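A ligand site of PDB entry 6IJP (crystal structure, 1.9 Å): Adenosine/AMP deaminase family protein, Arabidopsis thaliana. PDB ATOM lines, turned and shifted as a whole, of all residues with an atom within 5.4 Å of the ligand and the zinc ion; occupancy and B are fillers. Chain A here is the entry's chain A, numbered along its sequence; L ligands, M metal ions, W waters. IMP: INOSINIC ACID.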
ATOM      1  N   HIS A  34     -15.148   7.438  23.790  1.00  0.00           N
ATOM      2  CA  HIS A  34     -15.759   8.413  22.880  1.00  0.00           C
ATOM      3  C   HIS A  34     -17.246   8.542  23.229  1.00  0.00           C
ATOM      4  O   HIS A  34     -18.123   7.849  22.695  1.00  0.00           O
ATOM      5  CB  HIS A  34     -15.503   8.006  21.432  1.00  0.00           C
ATOM      6  CG  HIS A  34     -15.929   9.019  20.395  1.00  0.00           C
ATOM      7  ND1 HIS A  34     -15.196   9.249  19.250  1.00  0.00           N
ATOM      8  CD2 HIS A  34     -17.039   9.807  20.294  1.00  0.00           C
ATOM      9  CE1 HIS A  34     -15.819  10.150  18.490  1.00  0.00           C
ATOM     10  NE2 HIS A  34     -16.945  10.491  19.092  1.00  0.00           N
ATOM     11  N   HIS A  36     -19.897  11.858  24.049  1.00  0.00           N
ATOM     12  CA  HIS A  36     -20.173  13.284  24.235  1.00  0.00           C
ATOM     13  C   HIS A  36     -21.192  13.492  25.344  1.00  0.00           C
ATOM     14  O   HIS A  36     -22.241  12.813  25.381  1.00  0.00           O
ATOM     15  CB  HIS A  36     -20.714  13.914  22.924  1.00  0.00           C
ATOM     16  CG  HIS A  36     -19.861  13.715  21.717  1.00  0.00           C
ATOM     17  ND1 HIS A  36     -18.929  14.638  21.290  1.00  0.00           N
ATOM     18  CD2 HIS A  36     -19.846  12.716  20.776  1.00  0.00           C
ATOM     19  CE1 HIS A  36     -18.361  14.213  20.158  1.00  0.00           C
ATOM     20  NE2 HIS A  36     -18.898  13.050  19.844  1.00  0.00           N
ATOM     21  N   LEU A  37     -20.888  14.426  26.264  1.00  0.00           N
ATOM     22  CA  LEU A  37     -21.752  14.697  27.410  1.00  0.00           C
ATOM     23  C   LEU A  37     -23.199  14.964  26.988  1.00  0.00           C
ATOM     24  O   LEU A  37     -24.135  14.280  27.435  1.00  0.00           O
ATOM     25  CB  LEU A  37     -21.160  15.878  28.223  1.00  0.00           C
ATOM     26  CG  LEU A  37     -22.022  16.361  29.401  1.00  0.00           C
ATOM     27  CD1 LEU A  37     -22.330  15.219  30.416  1.00  0.00           C
ATOM     28  CD2 LEU A  37     -21.371  17.577  30.047  1.00  0.00           C
ATOM     29  N   ASN A  38     -23.400  15.951  26.109  1.00  0.00           N
ATOM     30  CA  ASN A  38     -24.788  16.327  25.783  1.00  0.00           C
ATOM     31  C   ASN A  38     -25.434  15.376  24.778  1.00  0.00           C
ATOM     32  O   ASN A  38     -26.611  15.567  24.448  1.00  0.00           O
ATOM     33  CB  ASN A  38     -24.847  17.770  25.287  1.00  0.00           C
ATOM     34  CG  ASN A  38     -24.723  18.787  26.435  1.00  0.00           C
ATOM     35  OD1 ASN A  38     -25.721  19.161  27.044  1.00  0.00           O
ATOM     36  ND2 ASN A  38     -23.495  19.209  26.750  1.00  0.00           N
ATOM     37  N   GLY A  39     -24.716  14.366  24.295  1.00  0.00           N
ATOM     38  CA  GLY A  39     -25.269  13.267  23.523  1.00  0.00           C
ATOM     39  C   GLY A  39     -25.613  12.068  24.368  1.00  0.00           C
ATOM     40  O   GLY A  39     -26.131  11.072  23.856  1.00  0.00           O
ATOM     41  N   LEU A  75     -27.076  12.221   9.449  1.00  0.00           N
ATOM     42  CA  LEU A  75     -25.957  13.095   9.796  1.00  0.00           C
ATOM     43  C   LEU A  75     -26.370  14.575   9.843  1.00  0.00           C
ATOM     44  O   LEU A  75     -26.176  15.241  10.874  1.00  0.00           O
ATOM     45  CB  LEU A  75     -24.808  12.911   8.804  1.00  0.00           C
ATOM     46  CG  LEU A  75     -23.489  13.449   9.351  1.00  0.00           C
ATOM     47  CD1 LEU A  75     -23.081  12.758  10.645  1.00  0.00           C
ATOM     48  CD2 LEU A  75     -22.436  13.256   8.311  1.00  0.00           C
ATOM     49  N   VAL A  78     -28.958  15.052  12.835  1.00  0.00           N
ATOM     50  CA  VAL A  78     -28.354  14.989  14.170  1.00  0.00           C
ATOM     51  C   VAL A  78     -27.909  16.382  14.639  1.00  0.00           C
ATOM     52  O   VAL A  78     -28.041  16.702  15.829  1.00  0.00           O
ATOM     53  CB  VAL A  78     -27.183  13.994  14.161  1.00  0.00           C
ATOM     54  CG1 VAL A  78     -26.341  14.177  15.391  1.00  0.00           C
ATOM     55  CG2 VAL A  78     -27.703  12.597  14.160  1.00  0.00           C
ATOM     56  N   PHE A  79     -27.354  17.213  13.748  1.00  0.00           N
ATOM     57  CA  PHE A  79     -26.833  18.490  14.242  1.00  0.00           C
ATOM     58  C   PHE A  79     -27.951  19.505  14.513  1.00  0.00           C
ATOM     59  O   PHE A  79     -27.795  20.383  15.382  1.00  0.00           O
ATOM     60  CB  PHE A  79     -25.762  19.012  13.264  1.00  0.00           C
ATOM     61  CG  PHE A  79     -24.542  18.127  13.251  1.00  0.00           C
ATOM     62  CD1 PHE A  79     -23.647  18.131  14.338  1.00  0.00           C
ATOM     63  CD2 PHE A  79     -24.355  17.207  12.242  1.00  0.00           C
ATOM     64  CE1 PHE A  79     -22.552  17.278  14.369  1.00  0.00           C
ATOM     65  CE2 PHE A  79     -23.260  16.346  12.254  1.00  0.00           C
ATOM     66  CZ  PHE A  79     -22.362  16.376  13.320  1.00  0.00           C
ATOM     67  N   PHE A  82     -28.786  18.529  18.009  1.00  0.00           N
ATOM     68  CA  PHE A  82     -27.885  19.084  19.032  1.00  0.00           C
ATOM     69  C   PHE A  82     -28.174  20.556  19.286  1.00  0.00           C
ATOM     70  O   PHE A  82     -28.090  21.012  20.438  1.00  0.00           O
ATOM     71  CB  PHE A  82     -26.417  18.885  18.658  1.00  0.00           C
ATOM     72  CG  PHE A  82     -25.934  17.492  18.866  1.00  0.00           C
ATOM     73  CD1 PHE A  82     -26.082  16.887  20.101  1.00  0.00           C
ATOM     74  CD2 PHE A  82     -25.356  16.755  17.830  1.00  0.00           C
ATOM     75  CE1 PHE A  82     -25.647  15.586  20.316  1.00  0.00           C
ATOM     76  CE2 PHE A  82     -24.939  15.444  18.059  1.00  0.00           C
ATOM     77  CZ  PHE A  82     -25.102  14.876  19.312  1.00  0.00           C
ATOM     78  N   HIS A  86     -28.919  21.792  23.082  1.00  0.00           N
ATOM     79  CA  HIS A  86     -28.154  22.850  23.738  1.00  0.00           C
ATOM     80  C   HIS A  86     -29.050  23.977  24.208  1.00  0.00           C
ATOM     81  O   HIS A  86     -28.712  24.666  25.184  1.00  0.00           O
ATOM     82  CB  HIS A  86     -27.095  23.394  22.794  1.00  0.00           C
ATOM     83  CG  HIS A  86     -25.942  22.452  22.601  1.00  0.00           C
ATOM     84  ND1 HIS A  86     -25.163  22.456  21.473  1.00  0.00           N
ATOM     85  CD2 HIS A  86     -25.455  21.480  23.404  1.00  0.00           C
ATOM     86  CE1 HIS A  86     -24.229  21.528  21.580  1.00  0.00           C
ATOM     87  NE2 HIS A  86     -24.372  20.920  22.751  1.00  0.00           N
ATOM     88  N   ARG A 117     -16.137  13.573  26.809  1.00  0.00           N
ATOM     89  CA  ARG A 117     -15.773  14.779  26.080  1.00  0.00           C
ATOM     90  C   ARG A 117     -16.952  15.745  26.048  1.00  0.00           C
ATOM     91  O   ARG A 117     -18.120  15.319  26.014  1.00  0.00           O
ATOM     92  CB  ARG A 117     -15.311  14.483  24.648  1.00  0.00           C
ATOM     93  CG  ARG A 117     -16.320  13.814  23.760  1.00  0.00           C
ATOM     94  CD  ARG A 117     -15.638  13.410  22.369  1.00  0.00           C
ATOM     95  NE  ARG A 117     -14.726  12.263  22.545  1.00  0.00           N
ATOM     96  CZ  ARG A 117     -13.928  11.802  21.597  1.00  0.00           C
ATOM     97  NH1 ARG A 117     -13.875  12.432  20.397  1.00  0.00           N
ATOM     98  NH2 ARG A 117     -13.194  10.698  21.823  1.00  0.00           N
ATOM     99  N   THR A 118     -16.636  17.023  26.122  1.00  0.00           N
ATOM    100  CA  THR A 118     -17.704  18.000  25.997  1.00  0.00           C
ATOM    101  C   THR A 118     -17.137  19.303  25.442  1.00  0.00           C
ATOM    102  O   THR A 118     -15.960  19.615  25.651  1.00  0.00           O
ATOM    103  CB  THR A 118     -18.444  18.252  27.322  1.00  0.00           C
ATOM    104  OG1 THR A 118     -19.594  19.068  27.070  1.00  0.00           O
ATOM    105  CG2 THR A 118     -17.510  18.923  28.394  1.00  0.00           C
ATOM    106  N   THR A 119     -17.997  20.015  24.709  1.00  0.00           N
ATOM    107  CA  THR A 119     -17.687  21.327  24.164  1.00  0.00           C
ATOM    108  C   THR A 119     -17.947  22.387  25.235  1.00  0.00           C
ATOM    109  O   THR A 119     -19.110  22.563  25.646  1.00  0.00           O
ATOM    110  CB  THR A 119     -18.547  21.600  22.951  1.00  0.00           C
ATOM    111  OG1 THR A 119     -18.553  20.466  22.045  1.00  0.00           O
ATOM    112  CG2 THR A 119     -17.995  22.834  22.208  1.00  0.00           C
ATOM    113  N   LYS A 121     -19.000  25.839  26.644  1.00  0.00           N
ATOM    114  CA  LYS A 121     -19.942  26.771  26.038  1.00  0.00           C
ATOM    115  C   LYS A 121     -19.788  28.151  26.647  1.00  0.00           C
ATOM    116  O   LYS A 121     -19.544  28.290  27.851  1.00  0.00           O
ATOM    117  CB  LYS A 121     -21.417  26.357  26.243  1.00  0.00           C
ATOM    118  CG  LYS A 121     -21.804  24.919  25.845  1.00  0.00           C
ATOM    119  CD  LYS A 121     -21.567  24.664  24.400  1.00  0.00           C
ATOM    120  CE  LYS A 121     -22.092  23.246  23.997  1.00  0.00           C
ATOM    121  NZ  LYS A 121     -21.944  22.147  25.041  1.00  0.00           N
ATOM    122  N   TYR A 133     -18.618  26.834  32.555  1.00  0.00           N
ATOM    123  CA  TYR A 133     -19.206  25.589  32.071  1.00  0.00           C
ATOM    124  C   TYR A 133     -18.399  24.403  32.567  1.00  0.00           C
ATOM    125  O   TYR A 133     -18.962  23.436  33.104  1.00  0.00           O
ATOM    126  CB  TYR A 133     -19.218  25.613  30.536  1.00  0.00           C
ATOM    127  CG  TYR A 133     -19.780  24.364  29.891  1.00  0.00           C
ATOM    128  CD1 TYR A 133     -21.081  24.339  29.425  1.00  0.00           C
ATOM    129  CD2 TYR A 133     -18.976  23.226  29.719  1.00  0.00           C
ATOM    130  CE1 TYR A 133     -21.608  23.201  28.842  1.00  0.00           C
ATOM    131  CE2 TYR A 133     -19.470  22.112  29.093  1.00  0.00           C
ATOM    132  CZ  TYR A 133     -20.790  22.093  28.657  1.00  0.00           C
ATOM    133  OH  TYR A 133     -21.251  20.967  28.035  1.00  0.00           O
ATOM    134  N   SER A 179     -13.744  19.453  23.898  1.00  0.00           N
ATOM    135  CA  SER A 179     -13.979  19.463  22.459  1.00  0.00           C
ATOM    136  C   SER A 179     -13.916  20.868  21.881  1.00  0.00           C
ATOM    137  O   SER A 179     -14.532  21.801  22.415  1.00  0.00           O
ATOM    138  CB  SER A 179     -15.337  18.894  22.077  1.00  0.00           C
ATOM    139  OG  SER A 179     -15.497  17.566  22.550  1.00  0.00           O
ATOM    140  N   ASP A 181     -15.358  22.750  18.632  1.00  0.00           N
ATOM    141  CA  ASP A 181     -16.428  22.551  17.660  1.00  0.00           C
ATOM    142  C   ASP A 181     -15.996  23.177  16.336  1.00  0.00           C
ATOM    143  O   ASP A 181     -15.394  24.254  16.316  1.00  0.00           O
ATOM    144  CB  ASP A 181     -17.707  23.216  18.197  1.00  0.00           C
ATOM    145  CG  ASP A 181     -18.949  23.004  17.320  1.00  0.00           C
ATOM    146  OD1 ASP A 181     -19.955  22.501  17.846  1.00  0.00           O
ATOM    147  OD2 ASP A 181     -18.980  23.397  16.132  1.00  0.00           O
ATOM    148  N   ARG A 183     -17.377  24.783  14.195  1.00  0.00           N
ATOM    149  CA  ARG A 183     -17.877  26.155  13.974  1.00  0.00           C
ATOM    150  C   ARG A 183     -16.956  27.253  14.524  1.00  0.00           C
ATOM    151  O   ARG A 183     -17.237  28.435  14.280  1.00  0.00           O
ATOM    152  CB  ARG A 183     -19.246  26.311  14.645  1.00  0.00           C
ATOM    153  CG  ARG A 183     -20.334  25.565  13.942  1.00  0.00           C
ATOM    154  CD  ARG A 183     -21.624  25.648  14.740  1.00  0.00           C
ATOM    155  NE  ARG A 183     -21.605  24.796  15.923  1.00  0.00           N
ATOM    156  CZ  ARG A 183     -22.674  24.572  16.681  1.00  0.00           C
ATOM    157  NH1 ARG A 183     -22.593  23.761  17.737  1.00  0.00           N
ATOM    158  NH2 ARG A 183     -23.827  25.172  16.388  1.00  0.00           N
ATOM    159  N   SER A 210     -14.569  18.100  17.017  1.00  0.00           N
ATOM    160  CA  SER A 210     -15.831  17.470  16.647  1.00  0.00           C
ATOM    161  C   SER A 210     -16.785  18.576  16.176  1.00  0.00           C
ATOM    162  O   SER A 210     -16.361  19.693  15.872  1.00  0.00           O
ATOM    163  CB  SER A 210     -16.387  16.619  17.817  1.00  0.00           C
ATOM    164  OG  SER A 210     -16.736  17.391  18.965  1.00  0.00           O
ATOM    165  N   GLY A 211     -18.081  18.257  16.100  1.00  0.00           N
ATOM    166  CA  GLY A 211     -19.040  19.165  15.472  1.00  0.00           C
ATOM    167  C   GLY A 211     -19.278  18.773  14.026  1.00  0.00           C
ATOM    168  O   GLY A 211     -18.772  17.781  13.517  1.00  0.00           O
ATOM    169  N   ASN A 212     -20.066  19.606  13.328  1.00  0.00           N
ATOM    170  CA  ASN A 212     -20.531  19.229  11.998  1.00  0.00           C
ATOM    171  C   ASN A 212     -19.372  19.089  10.999  1.00  0.00           C
ATOM    172  O   ASN A 212     -18.620  20.049  10.798  1.00  0.00           O
ATOM    173  CB  ASN A 212     -21.539  20.301  11.530  1.00  0.00           C
ATOM    174  CG  ASN A 212     -22.269  19.900  10.269  1.00  0.00           C
ATOM    175  OD1 ASN A 212     -21.791  19.084   9.505  1.00  0.00           O
ATOM    176  ND2 ASN A 212     -23.438  20.510  10.037  1.00  0.00           N
ATOM    177  N   PRO A 213     -19.150  17.901  10.425  1.00  0.00           N
ATOM    178  CA  PRO A 213     -17.977  17.706   9.556  1.00  0.00           C
ATOM    179  C   PRO A 213     -18.069  18.434   8.220  1.00  0.00           C
ATOM    180  O   PRO A 213     -17.071  18.464   7.489  1.00  0.00           O
ATOM    181  CB  PRO A 213     -17.956  16.196   9.311  1.00  0.00           C
ATOM    182  CG  PRO A 213     -19.380  15.783   9.515  1.00  0.00           C
ATOM    183  CD  PRO A 213     -19.910  16.670  10.619  1.00  0.00           C
ATOM    184  N   HIS A 238     -12.297  13.659  15.368  1.00  0.00           N
ATOM    185  CA  HIS A 238     -13.304  13.128  14.467  1.00  0.00           C
ATOM    186  C   HIS A 238     -12.773  13.202  13.033  1.00  0.00           C
ATOM    187  O   HIS A 238     -12.465  14.298  12.556  1.00  0.00           O
ATOM    188  CB  HIS A 238     -14.619  13.922  14.583  1.00  0.00           C
ATOM    189  CG  HIS A 238     -15.437  13.527  15.776  1.00  0.00           C
ATOM    190  ND1 HIS A 238     -15.018  13.760  17.079  1.00  0.00           N
ATOM    191  CD2 HIS A 238     -16.661  12.928  15.868  1.00  0.00           C
ATOM    192  CE1 HIS A 238     -15.943  13.318  17.924  1.00  0.00           C
ATOM    193  NE2 HIS A 238     -16.964  12.855  17.223  1.00  0.00           N
ATOM    194  N   GLU A 241     -15.719  11.525   8.828  1.00  0.00           N
ATOM    195  CA  GLU A 241     -17.162  11.301   9.019  1.00  0.00           C
ATOM    196  C   GLU A 241     -17.948  11.527   7.728  1.00  0.00           C
ATOM    197  O   GLU A 241     -19.052  10.985   7.590  1.00  0.00           O
ATOM    198  CB  GLU A 241     -17.734  12.229  10.085  1.00  0.00           C
ATOM    199  CG  GLU A 241     -17.209  12.030  11.488  1.00  0.00           C
ATOM    200  CD  GLU A 241     -17.985  12.955  12.451  1.00  0.00           C
ATOM    201  OE1 GLU A 241     -18.930  12.467  13.110  1.00  0.00           O
ATOM    202  OE2 GLU A 241     -17.677  14.157  12.503  1.00  0.00           O
ATOM    203  N   HIS A 261     -14.018   7.300  14.237  1.00  0.00           N
ATOM    204  CA  HIS A 261     -14.851   6.855  13.092  1.00  0.00           C
ATOM    205  C   HIS A 261     -14.184   6.379  11.828  1.00  0.00           C
ATOM    206  O   HIS A 261     -14.275   5.157  11.543  1.00  0.00           O
ATOM    207  CB  HIS A 261     -15.841   7.952  12.754  1.00  0.00           C
ATOM    208  CG  HIS A 261     -16.685   8.234  13.917  1.00  0.00           C
ATOM    209  ND1 HIS A 261     -17.001   7.218  14.783  1.00  0.00           N
ATOM    210  CD2 HIS A 261     -17.157   9.382  14.458  1.00  0.00           C
ATOM    211  CE1 HIS A 261     -17.679   7.719  15.788  1.00  0.00           C
ATOM    212  NE2 HIS A 261     -17.792   9.028  15.620  1.00  0.00           N
ATOM    213  N   SER A 286     -24.014   4.577  16.144  1.00  0.00           N
ATOM    214  CA  SER A 286     -23.968   5.922  15.590  1.00  0.00           C
ATOM    215  C   SER A 286     -23.722   5.890  14.064  1.00  0.00           C
ATOM    216  O   SER A 286     -24.455   6.516  13.288  1.00  0.00           O
ATOM    217  CB  SER A 286     -22.895   6.713  16.329  1.00  0.00           C
ATOM    218  OG  SER A 286     -22.626   7.917  15.678  1.00  0.00           O
ATOM    219  N   ASP A 316     -20.482   6.974  21.417  1.00  0.00           N
ATOM    220  CA  ASP A 316     -20.600   8.258  20.729  1.00  0.00           C
ATOM    221  C   ASP A 316     -21.631   9.152  21.437  1.00  0.00           C
ATOM    222  O   ASP A 316     -21.278  10.153  22.058  1.00  0.00           O
ATOM    223  CB  ASP A 316     -20.946   8.074  19.231  1.00  0.00           C
ATOM    224  CG  ASP A 316     -20.573   9.282  18.393  1.00  0.00           C
ATOM    225  OD1 ASP A 316     -19.950  10.231  18.944  1.00  0.00           O
ATOM    226  OD2 ASP A 316     -20.913   9.312  17.175  1.00  0.00           O
ATOM    227  N   ASP A 317     -22.923   8.799  21.333  1.00  0.00           N
ATOM    228  CA  ASP A 317     -24.016   9.582  21.915  1.00  0.00           C
ATOM    229  C   ASP A 317     -25.072   8.570  22.359  1.00  0.00           C
ATOM    230  O   ASP A 317     -26.024   8.314  21.636  1.00  0.00           O
ATOM    231  CB  ASP A 317     -24.640  10.577  20.921  1.00  0.00           C
ATOM    232  CG  ASP A 317     -23.639  11.559  20.382  1.00  0.00           C
ATOM    233  OD1 ASP A 317     -23.340  12.519  21.097  1.00  0.00           O
ATOM    234  OD2 ASP A 317     -23.167  11.397  19.219  1.00  0.00           O
ATOM    235  N   PHE A 321     -28.680   8.085  20.410  1.00  0.00           N
ATOM    236  CA  PHE A 321     -28.789   6.889  19.574  1.00  0.00           C
ATOM    237  C   PHE A 321     -29.381   5.698  20.311  1.00  0.00           C
ATOM    238  O   PHE A 321     -29.366   4.586  19.773  1.00  0.00           O
ATOM    239  CB  PHE A 321     -27.428   6.493  18.969  1.00  0.00           C
ATOM    240  CG  PHE A 321     -26.915   7.497  17.985  1.00  0.00           C
ATOM    241  CD1 PHE A 321     -27.599   7.728  16.809  1.00  0.00           C
ATOM    242  CD2 PHE A 321     -25.741   8.199  18.229  1.00  0.00           C
ATOM    243  CE1 PHE A 321     -27.147   8.657  15.890  1.00  0.00           C
ATOM    244  CE2 PHE A 321     -25.287   9.177  17.322  1.00  0.00           C
ATOM    245  CZ  PHE A 321     -25.988   9.395  16.152  1.00  0.00           C
HETATM  246  P   IMP L   1     -21.399  18.478  23.968  1.00  0.00           P
HETATM  247  O1P IMP L   1     -20.016  18.794  23.469  1.00  0.00           O
HETATM  248  O2P IMP L   1     -21.327  17.990  25.389  1.00  0.00           O
HETATM  249  O3P IMP L   1     -22.219  19.737  23.712  1.00  0.00           O
HETATM  250  O5' IMP L   1     -22.008  17.233  23.170  1.00  0.00           O
HETATM  251  C5' IMP L   1     -22.668  17.465  21.928  1.00  0.00           C
HETATM  252  C4' IMP L   1     -21.696  17.867  20.850  1.00  0.00           C
HETATM  253  O4' IMP L   1     -20.848  16.733  20.502  1.00  0.00           O
HETATM  254  C3' IMP L   1     -22.356  18.265  19.529  1.00  0.00           C
HETATM  255  O3' IMP L   1     -22.763  19.640  19.532  1.00  0.00           O
HETATM  256  C2' IMP L   1     -21.297  17.933  18.470  1.00  0.00           C
HETATM  257  O2' IMP L   1     -20.433  19.027  18.233  1.00  0.00           O
HETATM  258  C1' IMP L   1     -20.520  16.773  19.129  1.00  0.00           C
HETATM  259  N9  IMP L   1     -20.941  15.510  18.530  1.00  0.00           N
HETATM  260  C8  IMP L   1     -21.812  14.582  19.045  1.00  0.00           C
HETATM  261  N7  IMP L   1     -21.932  13.597  18.111  1.00  0.00           N
HETATM  262  C5  IMP L   1     -21.170  13.914  17.028  1.00  0.00           C
HETATM  263  C6  IMP L   1     -20.939  13.278  15.793  1.00  0.00           C
HETATM  264  O6  IMP L   1     -21.658  12.329  15.406  1.00  0.00           O
HETATM  265  N1  IMP L   1     -20.074  13.899  14.908  1.00  0.00           N
HETATM  266  C2  IMP L   1     -19.442  15.083  15.189  1.00  0.00           C
HETATM  267  N3  IMP L   1     -19.705  15.710  16.395  1.00  0.00           N
HETATM  268  C4  IMP L   1     -20.545  15.121  17.289  1.00  0.00           C
HETATM  269 ZN    ZN M   1     -18.534  11.707  18.207  1.00  0.00          ZN
HETATM  270  O   HOH W   1     -19.254  11.074  16.262  1.00  0.00           O
HETATM  271  O   HOH W   2     -20.879  21.573  20.318  1.00  0.00           O
HETATM  272  O   HOH W   3     -18.158  16.869  22.728  1.00  0.00           O
HETATM  273  O   HOH W   4     -22.698  20.614  16.644  1.00  0.00           O
HETATM  274  O   HOH W   5     -18.222  19.696  19.361  1.00  0.00           O
HETATM  275  O   HOH W   6     -21.224  10.717  12.796  1.00  0.00           O
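A ring nitrogen (ND1) of His 36 is in hydrogen-bond range of an oxygen (O4') of the ligand, 2.9 Å away.
The side-chain carboxylate (OE1) of Glu 241 sits at hydrogen-bond distance from a nitrogen (N1) of the ligand.
A ring nitrogen (NE2) of His 86 sits at hydrogen-bond distance from an oxygen (O3P) of the ligand.
An oxygen (O1P) of the ligand sits at hydrogen-bond distance from the backbone NH (N) of Thr 119 (2.7 Å).
An oxygen (O1P) of the ligand sits at hydrogen-bond distance from the side-chain hydroxyl of Thr 119 (2.6 Å).
O2P of the ligand sits at hydrogen-bond distance from OG1 of Thr 118 (2.6 Å).
A nitrogen (N7) of the ligand is in hydrogen-bond range of the side-chain carboxylate (OD2) of Asp 317, 2.8 Å away.
The side-chain amino group of Lys 121 is in salt-bridge range of an oxygen (O3P) of the ligand (2.8 Å).
O2P of the ligand sits at hydrogen-bond distance from N of Asn 38, 3.0 Å away.
The side-chain amide nitrogen (ND2) of Asn 38 is in hydrogen-bond range of an oxygen (O2P) of the ligand (2.8 Å).
The backbone NH (N) of Gly 211 lies within hydrogen-bond range of a nitrogen (N3) of the ligand, at 3.0 Å.
A ring nitrogen (NE2) of His 261 is in hydrogen-bond range of the side-chain carboxylate of Asp 316, at 3.5 Å.
OD2 of Asp 316 is in hydrogen-bond range of OG of Ser 286 (2.7 Å).
The backbone carbonyl oxygen (O) of Phe 82 sits close to a ring nitrogen (ND1) of His 86, at 3.4 Å.
The backbone carbonyl oxygen (O) of Thr 118 is in hydrogen-bond range of the backbone NH (N) of Ser 179.
The side-chain hydroxyl of Tyr 133 lies within hydrogen-bond range of the side-chain amino group of Lys 121 (3.3 Å).
ND2 of Asn 38 lies within hydrogen-bond range of OH of Tyr 133, at 3.1 Å.
NH1 of Arg 183 lies within salt-bridge range of OD1 of Asp 181 (2.9 Å).
The backbone NH (N) of Leu 37 is in hydrogen-bond range of the backbone carbonyl oxygen (O) of Arg 117 (2.9 Å).
Merely in contact with the ligand: Leu 37 (3.5 Å), Phe 79 (3.7 Å), Phe 82 (3.3 Å), Tyr 133 (3.98 Å), Asp 181 (3.5 Å) and Ser 210 (3.7 Å).
Hydrophobic or aromatic side chains within 4 Å of the ligand: His 36, Leu 37, Phe 79, Phe 82, His 86 and His 238.
17 residues have an atom within 4 Å of the ligand: His 36, Leu 37, Asn 38, Phe 79, Phe 82, His 86, Thr 118, Thr 119, Lys 121, Tyr 133, Asp 181, Ser 210, Gly 211, His 238, Glu 241, Asp 316 and Asp 317.
The nearest printed residue that does not touch the ligand is Gly 39 (4.1 Å).
Merely in contact with the zinc ion: His 261.
The nearest printed residue that does not touch the zinc ion is Asp 317 (4.8 Å).
The zinc ion is bound by NE2 of His 36, water W1, OD1 of Asp 316, NE2 of His 238 and NE2 of His 34.
Water W5 lies within hydrogen-bond range of O2' of the ligand (2.6 Å), OG of Ser 210 (2.8 Å) and OG1 of Thr 119 (2.8 Å).
Water W3 lies within hydrogen-bond range of the side-chain hydroxyl of Ser 179 (2.8 Å), a ring nitrogen (ND1) of His 36 (2.8 Å) and an oxygen (O1P) of the ligand (2.8 Å).
Water W2 lies within hydrogen-bond range of the side-chain carboxylate of Asp 181 (2.8 Å), an oxygen (O3') of the ligand (2.8 Å) and the side-chain hydroxyl of Thr 119 (3.1 Å).
Water W4 lies within hydrogen-bond range of an oxygen (O3') of the ligand (3.0 Å) and the guanidinium group of Arg 183 (3.3 Å).
Water W6 lies within hydrogen-bond range of the side-chain carboxylate of Glu 241 (2.9 Å) and an oxygen (O6) of the ligand (3.1 Å).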
